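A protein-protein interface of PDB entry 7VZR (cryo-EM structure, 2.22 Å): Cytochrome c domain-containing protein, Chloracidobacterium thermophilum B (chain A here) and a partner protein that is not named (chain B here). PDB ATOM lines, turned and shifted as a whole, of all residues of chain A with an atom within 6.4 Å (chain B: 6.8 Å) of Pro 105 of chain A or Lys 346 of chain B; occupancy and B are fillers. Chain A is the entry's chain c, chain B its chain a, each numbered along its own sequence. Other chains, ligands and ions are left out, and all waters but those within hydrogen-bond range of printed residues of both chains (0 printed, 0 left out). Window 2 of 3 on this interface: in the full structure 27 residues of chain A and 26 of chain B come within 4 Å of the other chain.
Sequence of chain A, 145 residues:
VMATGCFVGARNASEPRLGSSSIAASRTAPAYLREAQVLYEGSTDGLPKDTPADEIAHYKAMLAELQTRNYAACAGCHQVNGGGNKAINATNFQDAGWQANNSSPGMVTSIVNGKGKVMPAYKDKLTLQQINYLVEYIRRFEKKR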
ATOM      1  N   SER A 103     -23.972   0.087  -0.694  1.00  0.00           N
ATOM      2  CA  SER A 103     -23.375   1.404  -0.538  1.00  0.00           C
ATOM      3  C   SER A 103     -22.969   1.590   0.911  1.00  0.00           C
ATOM      4  O   SER A 103     -23.392   0.863   1.773  1.00  0.00           O
ATOM      5  CB  SER A 103     -24.237   2.577  -1.029  1.00  0.00           C
ATOM      6  OG  SER A 103     -25.307   2.971  -0.205  1.00  0.00           O
ATOM      7  N   SER A 104     -22.025   2.406   1.123  1.00  0.00           N
ATOM      8  CA  SER A 104     -21.533   2.737   2.448  1.00  0.00           C
ATOM      9  C   SER A 104     -22.587   3.430   3.280  1.00  0.00           C
ATOM     10  O   SER A 104     -22.797   3.010   4.396  1.00  0.00           O
ATOM     11  CB  SER A 104     -20.283   3.572   2.438  1.00  0.00           C
ATOM     12  OG  SER A 104     -19.327   3.132   1.599  1.00  0.00           O
ATOM     13  N   PRO A 105     -23.266   4.437   2.791  1.00  0.00           N
ATOM     14  CA  PRO A 105     -24.459   4.899   3.479  1.00  0.00           C
ATOM     15  C   PRO A 105     -25.451   3.809   3.838  1.00  0.00           C
ATOM     16  O   PRO A 105     -25.847   3.748   4.980  1.00  0.00           O
ATOM     17  CB  PRO A 105     -25.000   5.903   2.482  1.00  0.00           C
ATOM     18  CG  PRO A 105     -23.913   6.302   1.789  1.00  0.00           C
ATOM     19  CD  PRO A 105     -23.164   5.165   1.528  1.00  0.00           C
ATOM     20  N   GLY A 106     -25.773   2.897   2.930  1.00  0.00           N
ATOM     21  CA  GLY A 106     -26.699   1.837   3.248  1.00  0.00           C
ATOM     22  C   GLY A 106     -26.185   0.900   4.313  1.00  0.00           C
ATOM     23  O   GLY A 106     -26.915   0.573   5.229  1.00  0.00           O
ATOM     24  N   MET A 107     -24.924   0.526   4.239  1.00  0.00           N
ATOM     25  CA  MET A 107     -24.288  -0.370   5.195  1.00  0.00           C
ATOM     26  C   MET A 107     -24.448   0.071   6.642  1.00  0.00           C
ATOM     27  O   MET A 107     -24.539  -0.761   7.520  1.00  0.00           O
ATOM     28  CB  MET A 107     -22.821  -0.466   4.913  1.00  0.00           C
ATOM     29  CG  MET A 107     -22.220  -1.774   4.824  1.00  0.00           C
ATOM     30  SD  MET A 107     -20.522  -1.725   4.292  1.00  0.00           S
ATOM     31  CE  MET A 107     -20.012  -2.223   5.753  1.00  0.00           C
ATOM     32  N   VAL A 108     -24.286   1.367   6.893  1.00  0.00           N
ATOM     33  CA  VAL A 108     -24.476   2.058   8.151  1.00  0.00           C
ATOM     34  C   VAL A 108     -25.715   1.564   8.899  1.00  0.00           C
ATOM     35  O   VAL A 108     -25.594   1.100  10.008  1.00  0.00           O
ATOM     36  CB  VAL A 108     -24.527   3.592   7.922  1.00  0.00           C
ATOM     37  CG1 VAL A 108     -25.358   4.345   8.992  1.00  0.00           C
ATOM     38  CG2 VAL A 108     -23.166   4.157   7.852  1.00  0.00           C
ATOM     39  N   THR A 109     -26.897   1.603   8.281  1.00  0.00           N
ATOM     40  CA  THR A 109     -28.128   1.306   9.006  1.00  0.00           C
ATOM     41  C   THR A 109     -28.304  -0.162   9.304  1.00  0.00           C
ATOM     42  O   THR A 109     -28.820  -0.481  10.344  1.00  0.00           O
ATOM     43  CB  THR A 109     -29.414   1.846   8.329  1.00  0.00           C
ATOM     44  OG1 THR A 109     -29.703   1.222   7.085  1.00  0.00           O
ATOM     45  CG2 THR A 109     -29.406   3.370   8.233  1.00  0.00           C
ATOM     46  N   SER A 110     -27.743  -1.024   8.517  1.00  0.00           N
ATOM     47  CA  SER A 110     -27.676  -2.411   8.820  1.00  0.00           C
ATOM     48  C   SER A 110     -26.828  -2.722  10.051  1.00  0.00           C
ATOM     49  O   SER A 110     -27.264  -3.519  10.847  1.00  0.00           O
ATOM     50  CB  SER A 110     -27.227  -3.107   7.575  1.00  0.00           C
ATOM     51  OG  SER A 110     -26.878  -4.337   7.952  1.00  0.00           O
ATOM     52  N   ILE A 131     -19.689   3.881  13.999  1.00  0.00           N
ATOM     53  CA  ILE A 131     -20.201   3.024  12.943  1.00  0.00           C
ATOM     54  C   ILE A 131     -19.656   3.424  11.596  1.00  0.00           C
ATOM     55  O   ILE A 131     -19.280   2.564  10.809  1.00  0.00           O
ATOM     56  CB  ILE A 131     -21.738   2.982  12.970  1.00  0.00           C
ATOM     57  CG1 ILE A 131     -22.139   2.296  14.238  1.00  0.00           C
ATOM     58  CG2 ILE A 131     -22.309   2.261  11.808  1.00  0.00           C
ATOM     59  CD1 ILE A 131     -23.525   2.403  14.605  1.00  0.00           C
ATOM     60  N   ASN A 132     -19.530   4.733  11.351  1.00  0.00           N
ATOM     61  CA  ASN A 132     -18.898   5.270  10.148  1.00  0.00           C
ATOM     62  C   ASN A 132     -17.480   4.758   9.971  1.00  0.00           C
ATOM     63  O   ASN A 132     -17.127   4.269   8.904  1.00  0.00           O
ATOM     64  CB  ASN A 132     -18.880   6.790  10.163  1.00  0.00           C
ATOM     65  CG  ASN A 132     -20.174   7.397   9.966  1.00  0.00           C
ATOM     66  OD1 ASN A 132     -21.027   6.873   9.366  1.00  0.00           O
ATOM     67  ND2 ASN A 132     -20.340   8.529  10.511  1.00  0.00           N
ATOM     68  N   TYR A 133     -16.672   4.769  11.047  1.00  0.00           N
ATOM     69  CA  TYR A 133     -15.322   4.223  11.025  1.00  0.00           C
ATOM     70  C   TYR A 133     -15.294   2.745  10.659  1.00  0.00           C
ATOM     71  O   TYR A 133     -14.417   2.330   9.907  1.00  0.00           O
ATOM     72  CB  TYR A 133     -14.543   4.388  12.331  1.00  0.00           C
ATOM     73  CG  TYR A 133     -14.426   5.734  12.886  1.00  0.00           C
ATOM     74  CD1 TYR A 133     -14.709   6.854  12.138  1.00  0.00           C
ATOM     75  CD2 TYR A 133     -14.049   5.899  14.178  1.00  0.00           C
ATOM     76  CE1 TYR A 133     -14.609   8.051  12.617  1.00  0.00           C
ATOM     77  CE2 TYR A 133     -14.013   7.102  14.699  1.00  0.00           C
ATOM     78  CZ  TYR A 133     -14.292   8.186  13.902  1.00  0.00           C
ATOM     79  OH  TYR A 133     -14.180   9.412  14.403  1.00  0.00           O
ATOM     80  N   VAL A 135     -17.517   1.060   8.836  1.00  0.00           N
ATOM     81  CA  VAL A 135     -17.939   0.896   7.455  1.00  0.00           C
ATOM     82  C   VAL A 135     -16.716   1.103   6.558  1.00  0.00           C
ATOM     83  O   VAL A 135     -16.483   0.346   5.614  1.00  0.00           O
ATOM     84  CB  VAL A 135     -19.093   1.848   7.081  1.00  0.00           C
ATOM     85  CG1 VAL A 135     -19.313   1.857   5.637  1.00  0.00           C
ATOM     86  CG2 VAL A 135     -20.385   1.421   7.659  1.00  0.00           C
ATOM     87  N   GLU A 136     -15.876   2.051   6.927  1.00  0.00           N
ATOM     88  CA  GLU A 136     -14.618   2.314   6.248  1.00  0.00           C
ATOM     89  C   GLU A 136     -13.594   1.160   6.364  1.00  0.00           C
ATOM     90  O   GLU A 136     -13.079   0.681   5.358  1.00  0.00           O
ATOM     91  CB  GLU A 136     -14.023   3.630   6.772  1.00  0.00           C
ATOM     92  CG  GLU A 136     -14.666   4.848   6.398  1.00  0.00           C
ATOM     93  CD  GLU A 136     -15.003   4.950   4.996  1.00  0.00           C
ATOM     94  OE1 GLU A 136     -16.089   5.396   4.671  1.00  0.00           O
ATOM     95  OE2 GLU A 136     -14.206   4.618   4.149  1.00  0.00           O
ATOM     96  N   ARG A 139     -14.532  -1.854   4.211  1.00  0.00           N
ATOM     97  CA  ARG A 139     -14.296  -1.604   2.842  1.00  0.00           C
ATOM     98  C   ARG A 139     -12.972  -2.102   2.427  1.00  0.00           C
ATOM     99  O   ARG A 139     -12.840  -2.529   1.397  1.00  0.00           O
ATOM    100  CB  ARG A 139     -14.533  -0.193   2.452  1.00  0.00           C
ATOM    101  CG  ARG A 139     -15.938   0.220   2.486  1.00  0.00           C
ATOM    102  CD  ARG A 139     -16.624   0.376   1.242  1.00  0.00           C
ATOM    103  NE  ARG A 139     -17.375  -0.722   0.764  1.00  0.00           N
ATOM    104  CZ  ARG A 139     -18.624  -0.698   0.359  1.00  0.00           C
ATOM    105  NH1 ARG A 139     -19.378   0.280   0.518  1.00  0.00           N
ATOM    106  NH2 ARG A 139     -19.148  -1.766  -0.022  1.00  0.00           N
ATOM    107  N   ASN B 339     -13.613  10.715   5.445  1.00  0.00           N
ATOM    108  CA  ASN B 339     -14.855  10.458   6.073  1.00  0.00           C
ATOM    109  C   ASN B 339     -15.757  11.736   5.968  1.00  0.00           C
ATOM    110  O   ASN B 339     -16.102  12.293   6.882  1.00  0.00           O
ATOM    111  CB  ASN B 339     -14.575   9.721   7.476  1.00  0.00           C
ATOM    112  CG  ASN B 339     -15.734   9.563   8.370  1.00  0.00           C
ATOM    113  OD1 ASN B 339     -15.710   9.958   9.441  1.00  0.00           O
ATOM    114  ND2 ASN B 339     -16.693   8.992   7.943  1.00  0.00           N
ATOM    115  N   VAL B 340     -16.159  12.114   4.787  1.00  0.00           N
ATOM    116  CA  VAL B 340     -16.914  13.342   4.541  1.00  0.00           C
ATOM    117  C   VAL B 340     -18.377  13.199   4.941  1.00  0.00           C
ATOM    118  O   VAL B 340     -19.064  12.259   4.548  1.00  0.00           O
ATOM    119  CB  VAL B 340     -16.732  13.792   3.085  1.00  0.00           C
ATOM    120  CG1 VAL B 340     -17.767  14.751   2.620  1.00  0.00           C
ATOM    121  CG2 VAL B 340     -15.408  14.359   2.858  1.00  0.00           C
ATOM    122  N   ILE B 341     -18.834  14.035   5.837  1.00  0.00           N
ATOM    123  CA  ILE B 341     -20.170  13.943   6.361  1.00  0.00           C
ATOM    124  C   ILE B 341     -20.869  15.283   6.221  1.00  0.00           C
ATOM    125  O   ILE B 341     -20.395  16.292   6.740  1.00  0.00           O
ATOM    126  CB  ILE B 341     -20.156  13.425   7.806  1.00  0.00           C
ATOM    127  CG1 ILE B 341     -19.642  12.017   7.794  1.00  0.00           C
ATOM    128  CG2 ILE B 341     -21.453  13.339   8.359  1.00  0.00           C
ATOM    129  CD1 ILE B 341     -19.073  11.580   8.900  1.00  0.00           C
ATOM    130  N   ILE B 342     -21.969  15.309   5.516  1.00  0.00           N
ATOM    131  CA  ILE B 342     -22.736  16.526   5.279  1.00  0.00           C
ATOM    132  C   ILE B 342     -24.168  16.346   5.737  1.00  0.00           C
ATOM    133  O   ILE B 342     -24.861  15.513   5.184  1.00  0.00           O
ATOM    134  CB  ILE B 342     -22.726  16.956   3.792  1.00  0.00           C
ATOM    135  CG1 ILE B 342     -21.325  16.829   3.226  1.00  0.00           C
ATOM    136  CG2 ILE B 342     -23.364  18.321   3.613  1.00  0.00           C
ATOM    137  CD1 ILE B 342     -21.223  17.125   1.864  1.00  0.00           C
ATOM    138  N   TYR B 343     -24.631  17.280   6.560  1.00  0.00           N
ATOM    139  CA  TYR B 343     -25.933  17.320   7.207  1.00  0.00           C
ATOM    140  C   TYR B 343     -26.237  15.964   7.825  1.00  0.00           C
ATOM    141  O   TYR B 343     -27.313  15.429   7.730  1.00  0.00           O
ATOM    142  CB  TYR B 343     -27.018  17.818   6.230  1.00  0.00           C
ATOM    143  CG  TYR B 343     -28.293  18.252   6.872  1.00  0.00           C
ATOM    144  CD1 TYR B 343     -28.339  19.347   7.669  1.00  0.00           C
ATOM    145  CD2 TYR B 343     -29.419  17.436   6.797  1.00  0.00           C
ATOM    146  CE1 TYR B 343     -29.506  19.721   8.222  1.00  0.00           C
ATOM    147  CE2 TYR B 343     -30.551  17.777   7.369  1.00  0.00           C
ATOM    148  CZ  TYR B 343     -30.576  18.915   8.117  1.00  0.00           C
ATOM    149  OH  TYR B 343     -31.668  19.286   8.716  1.00  0.00           O
ATOM    150  N   GLY B 344     -25.244  15.437   8.458  1.00  0.00           N
ATOM    151  CA  GLY B 344     -25.174  14.100   8.948  1.00  0.00           C
ATOM    152  C   GLY B 344     -25.045  12.936   7.995  1.00  0.00           C
ATOM    153  O   GLY B 344     -25.488  11.894   8.379  1.00  0.00           O
ATOM    154  N   LYS B 345     -24.462  12.966   6.815  1.00  0.00           N
ATOM    155  CA  LYS B 345     -24.843  11.784   6.070  1.00  0.00           C
ATOM    156  C   LYS B 345     -23.827  10.739   5.619  1.00  0.00           C
ATOM    157  O   LYS B 345     -23.953   9.606   6.063  1.00  0.00           O
ATOM    158  CB  LYS B 345     -25.645  12.201   4.850  1.00  0.00           C
ATOM    159  CG  LYS B 345     -27.086  12.578   5.104  1.00  0.00           C
ATOM    160  CD  LYS B 345     -27.875  11.495   5.778  1.00  0.00           C
ATOM    161  CE  LYS B 345     -27.809  10.150   5.086  1.00  0.00           C
ATOM    162  NZ  LYS B 345     -28.308  10.205   3.743  1.00  0.00           N
ATOM    163  N   LYS B 346     -22.784  11.051   4.878  1.00  0.00           N
ATOM    164  CA  LYS B 346     -21.756  10.123   4.159  1.00  0.00           C
ATOM    165  C   LYS B 346     -22.028  10.195   2.732  1.00  0.00           C
ATOM    166  O   LYS B 346     -22.922   9.764   2.366  1.00  0.00           O
ATOM    167  CB  LYS B 346     -21.422   8.651   4.511  1.00  0.00           C
ATOM    168  CG  LYS B 346     -20.981   8.352   5.897  1.00  0.00           C
ATOM    169  CD  LYS B 346     -21.104   6.894   6.146  1.00  0.00           C
ATOM    170  CE  LYS B 346     -19.901   5.963   5.974  1.00  0.00           C
ATOM    171  NZ  LYS B 346     -18.615   6.496   6.317  1.00  0.00           N
ATOM    172  N   ILE B 347     -21.163  10.690   1.937  1.00  0.00           N
ATOM    173  CA  ILE B 347     -21.378  11.049   0.558  1.00  0.00           C
ATOM    174  C   ILE B 347     -20.687  10.042  -0.331  1.00  0.00           C
ATOM    175  O   ILE B 347     -19.547   9.700  -0.096  1.00  0.00           O
ATOM    176  CB  ILE B 347     -20.820  12.467   0.381  1.00  0.00           C
ATOM    177  CG1 ILE B 347     -21.491  13.413   1.385  1.00  0.00           C
ATOM    178  CG2 ILE B 347     -20.730  12.871  -1.056  1.00  0.00           C
ATOM    179  CD1 ILE B 347     -22.911  13.711   1.204  1.00  0.00           C
ATOM    180  N   VAL B 348     -21.332   9.632  -1.413  1.00  0.00           N
ATOM    181  CA  VAL B 348     -20.649   8.846  -2.433  1.00  0.00           C
ATOM    182  C   VAL B 348     -19.775   9.747  -3.284  1.00  0.00           C
ATOM    183  O   VAL B 348     -20.276  10.636  -3.937  1.00  0.00           O
ATOM    184  CB  VAL B 348     -21.633   8.056  -3.300  1.00  0.00           C
ATOM    185  CG1 VAL B 348     -20.873   7.219  -4.271  1.00  0.00           C
ATOM    186  CG2 VAL B 348     -22.423   7.196  -2.449  1.00  0.00           C
ATOM    187  N   PRO B 350     -17.329  12.280  -2.818  1.00  0.00           N
ATOM    188  CA  PRO B 350     -17.287  13.732  -2.660  1.00  0.00           C
ATOM    189  C   PRO B 350     -16.217  14.441  -3.452  1.00  0.00           C
ATOM    190  O   PRO B 350     -16.500  15.514  -3.922  1.00  0.00           O
ATOM    191  CB  PRO B 350     -17.081  13.869  -1.146  1.00  0.00           C
ATOM    192  CG  PRO B 350     -16.491  12.704  -0.795  1.00  0.00           C
ATOM    193  CD  PRO B 350     -17.053  11.660  -1.519  1.00  0.00           C
ATOM    194  N   TRP B 769     -32.001   9.676  -4.161  1.00  0.00           N
ATOM    195  CA  TRP B 769     -30.899   9.979  -3.346  1.00  0.00           C
ATOM    196  C   TRP B 769     -31.103  11.312  -2.728  1.00  0.00           C
ATOM    197  O   TRP B 769     -30.705  11.490  -1.672  1.00  0.00           O
ATOM    198  CB  TRP B 769     -29.556   9.693  -4.019  1.00  0.00           C
ATOM    199  CG  TRP B 769     -29.204   8.293  -4.008  1.00  0.00           C
ATOM    200  CD1 TRP B 769     -29.472   7.391  -4.941  1.00  0.00           C
ATOM    201  CD2 TRP B 769     -28.566   7.616  -2.997  1.00  0.00           C
ATOM    202  NE1 TRP B 769     -29.003   6.248  -4.629  1.00  0.00           N
ATOM    203  CE2 TRP B 769     -28.469   6.308  -3.401  1.00  0.00           C
ATOM    204  CE3 TRP B 769     -28.088   7.980  -1.749  1.00  0.00           C
ATOM    205  CZ2 TRP B 769     -27.869   5.337  -2.627  1.00  0.00           C
ATOM    206  CZ3 TRP B 769     -27.499   7.048  -1.009  1.00  0.00           C
ATOM    207  CH2 TRP B 769     -27.367   5.733  -1.466  1.00  0.00           C
ATOM    208  N   ASP B 859     -26.182  15.755  -4.388  1.00  0.00           N
ATOM    209  CA  ASP B 859     -26.616  14.467  -3.933  1.00  0.00           C
ATOM    210  C   ASP B 859     -25.464  13.452  -3.862  1.00  0.00           C
ATOM    211  O   ASP B 859     -25.526  12.560  -3.048  1.00  0.00           O
ATOM    212  CB  ASP B 859     -27.803  14.031  -4.792  1.00  0.00           C
ATOM    213  CG  ASP B 859     -27.470  13.382  -6.074  1.00  0.00           C
ATOM    214  OD1 ASP B 859     -26.406  13.377  -6.607  1.00  0.00           O
ATOM    215  OD2 ASP B 859     -28.348  12.852  -6.607  1.00  0.00           O
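The side-chain carboxylate (OE1) of Glu 136 of chain A lies within salt-bridge range of the side-chain amino group (NZ) of Lys 346 of chain B (3.2 Å).
OG of Ser 103 of chain A lies within hydrogen-bond range of N of Gly 106 of chain A (3.2 Å).
Among the printed residues, merely in contact across the chains: Asn 132 of chain A with Lys 346 of chain B (3.2 Å), Pro 105 of chain A with Lys 346 of chain B (3.6 Å), Ser 103 of chain A with Trp 769 of chain B (3.7 Å), Asn 132 of chain A with Ile 341 of chain B (3.7 Å), Asn 132 of chain A with Asn 339 of chain B (3.8 Å), Val 108 of chain A with Lys 346 of chain B (3.8 Å) and Tyr 133 of chain A with Asn 339 of chain B (3.9 Å).
Of chain B, only Lys 346 (3.6 Å) comes within 4 Å of Pro 105 of chain A. Lys 346 of chain B touches four residues of chain A. Of the printed residues of chain B, Asn 132 of chain A touches Asn 339 (3.8 Å), Ile 341 (3.7 Å) and Lys 346 (3.2 Å). Printed residues of chain B within 4 Å of Glu 136 of chain A: Lys 346 (3.2 Å). Printed residues of chain A within 4 Å of Trp 769 of chain B: Ser 103 (3.7 Å). Printed residues of chain A within 4 Å of Ile 341 of chain B: Asn 132. Printed residues of chain B within 4 Å of Tyr 133 of chain A: Asn 339. Arg 139 of chain A touches none of the printed residues of chain B. The nearest residue of chain B that does not touch Pro 105 of chain A is Trp 769 of chain B (4.4 Å). The nearest residue of chain A that does not touch Lys 346 of chain B is Val 135 of chain A (4.2 Å).
Of the 14 printed residues of chain A, 6 touch a printed residue of chain B. Hydrophobic or aromatic side chains of chain A within 4 Å of the printed part of chain B: Pro 105, Val 108 and Tyr 133. Hydrophobic or aromatic side chains of chain B within 4 Å of the printed part of chain A: Ile 341 and Trp 769. Among the printed residues, Asp or Glu carboxylates within 4 Å of a Lys or Arg side-chain nitrogen of the other chain: Glu 136 of chain A with Lys 346 of chain B.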
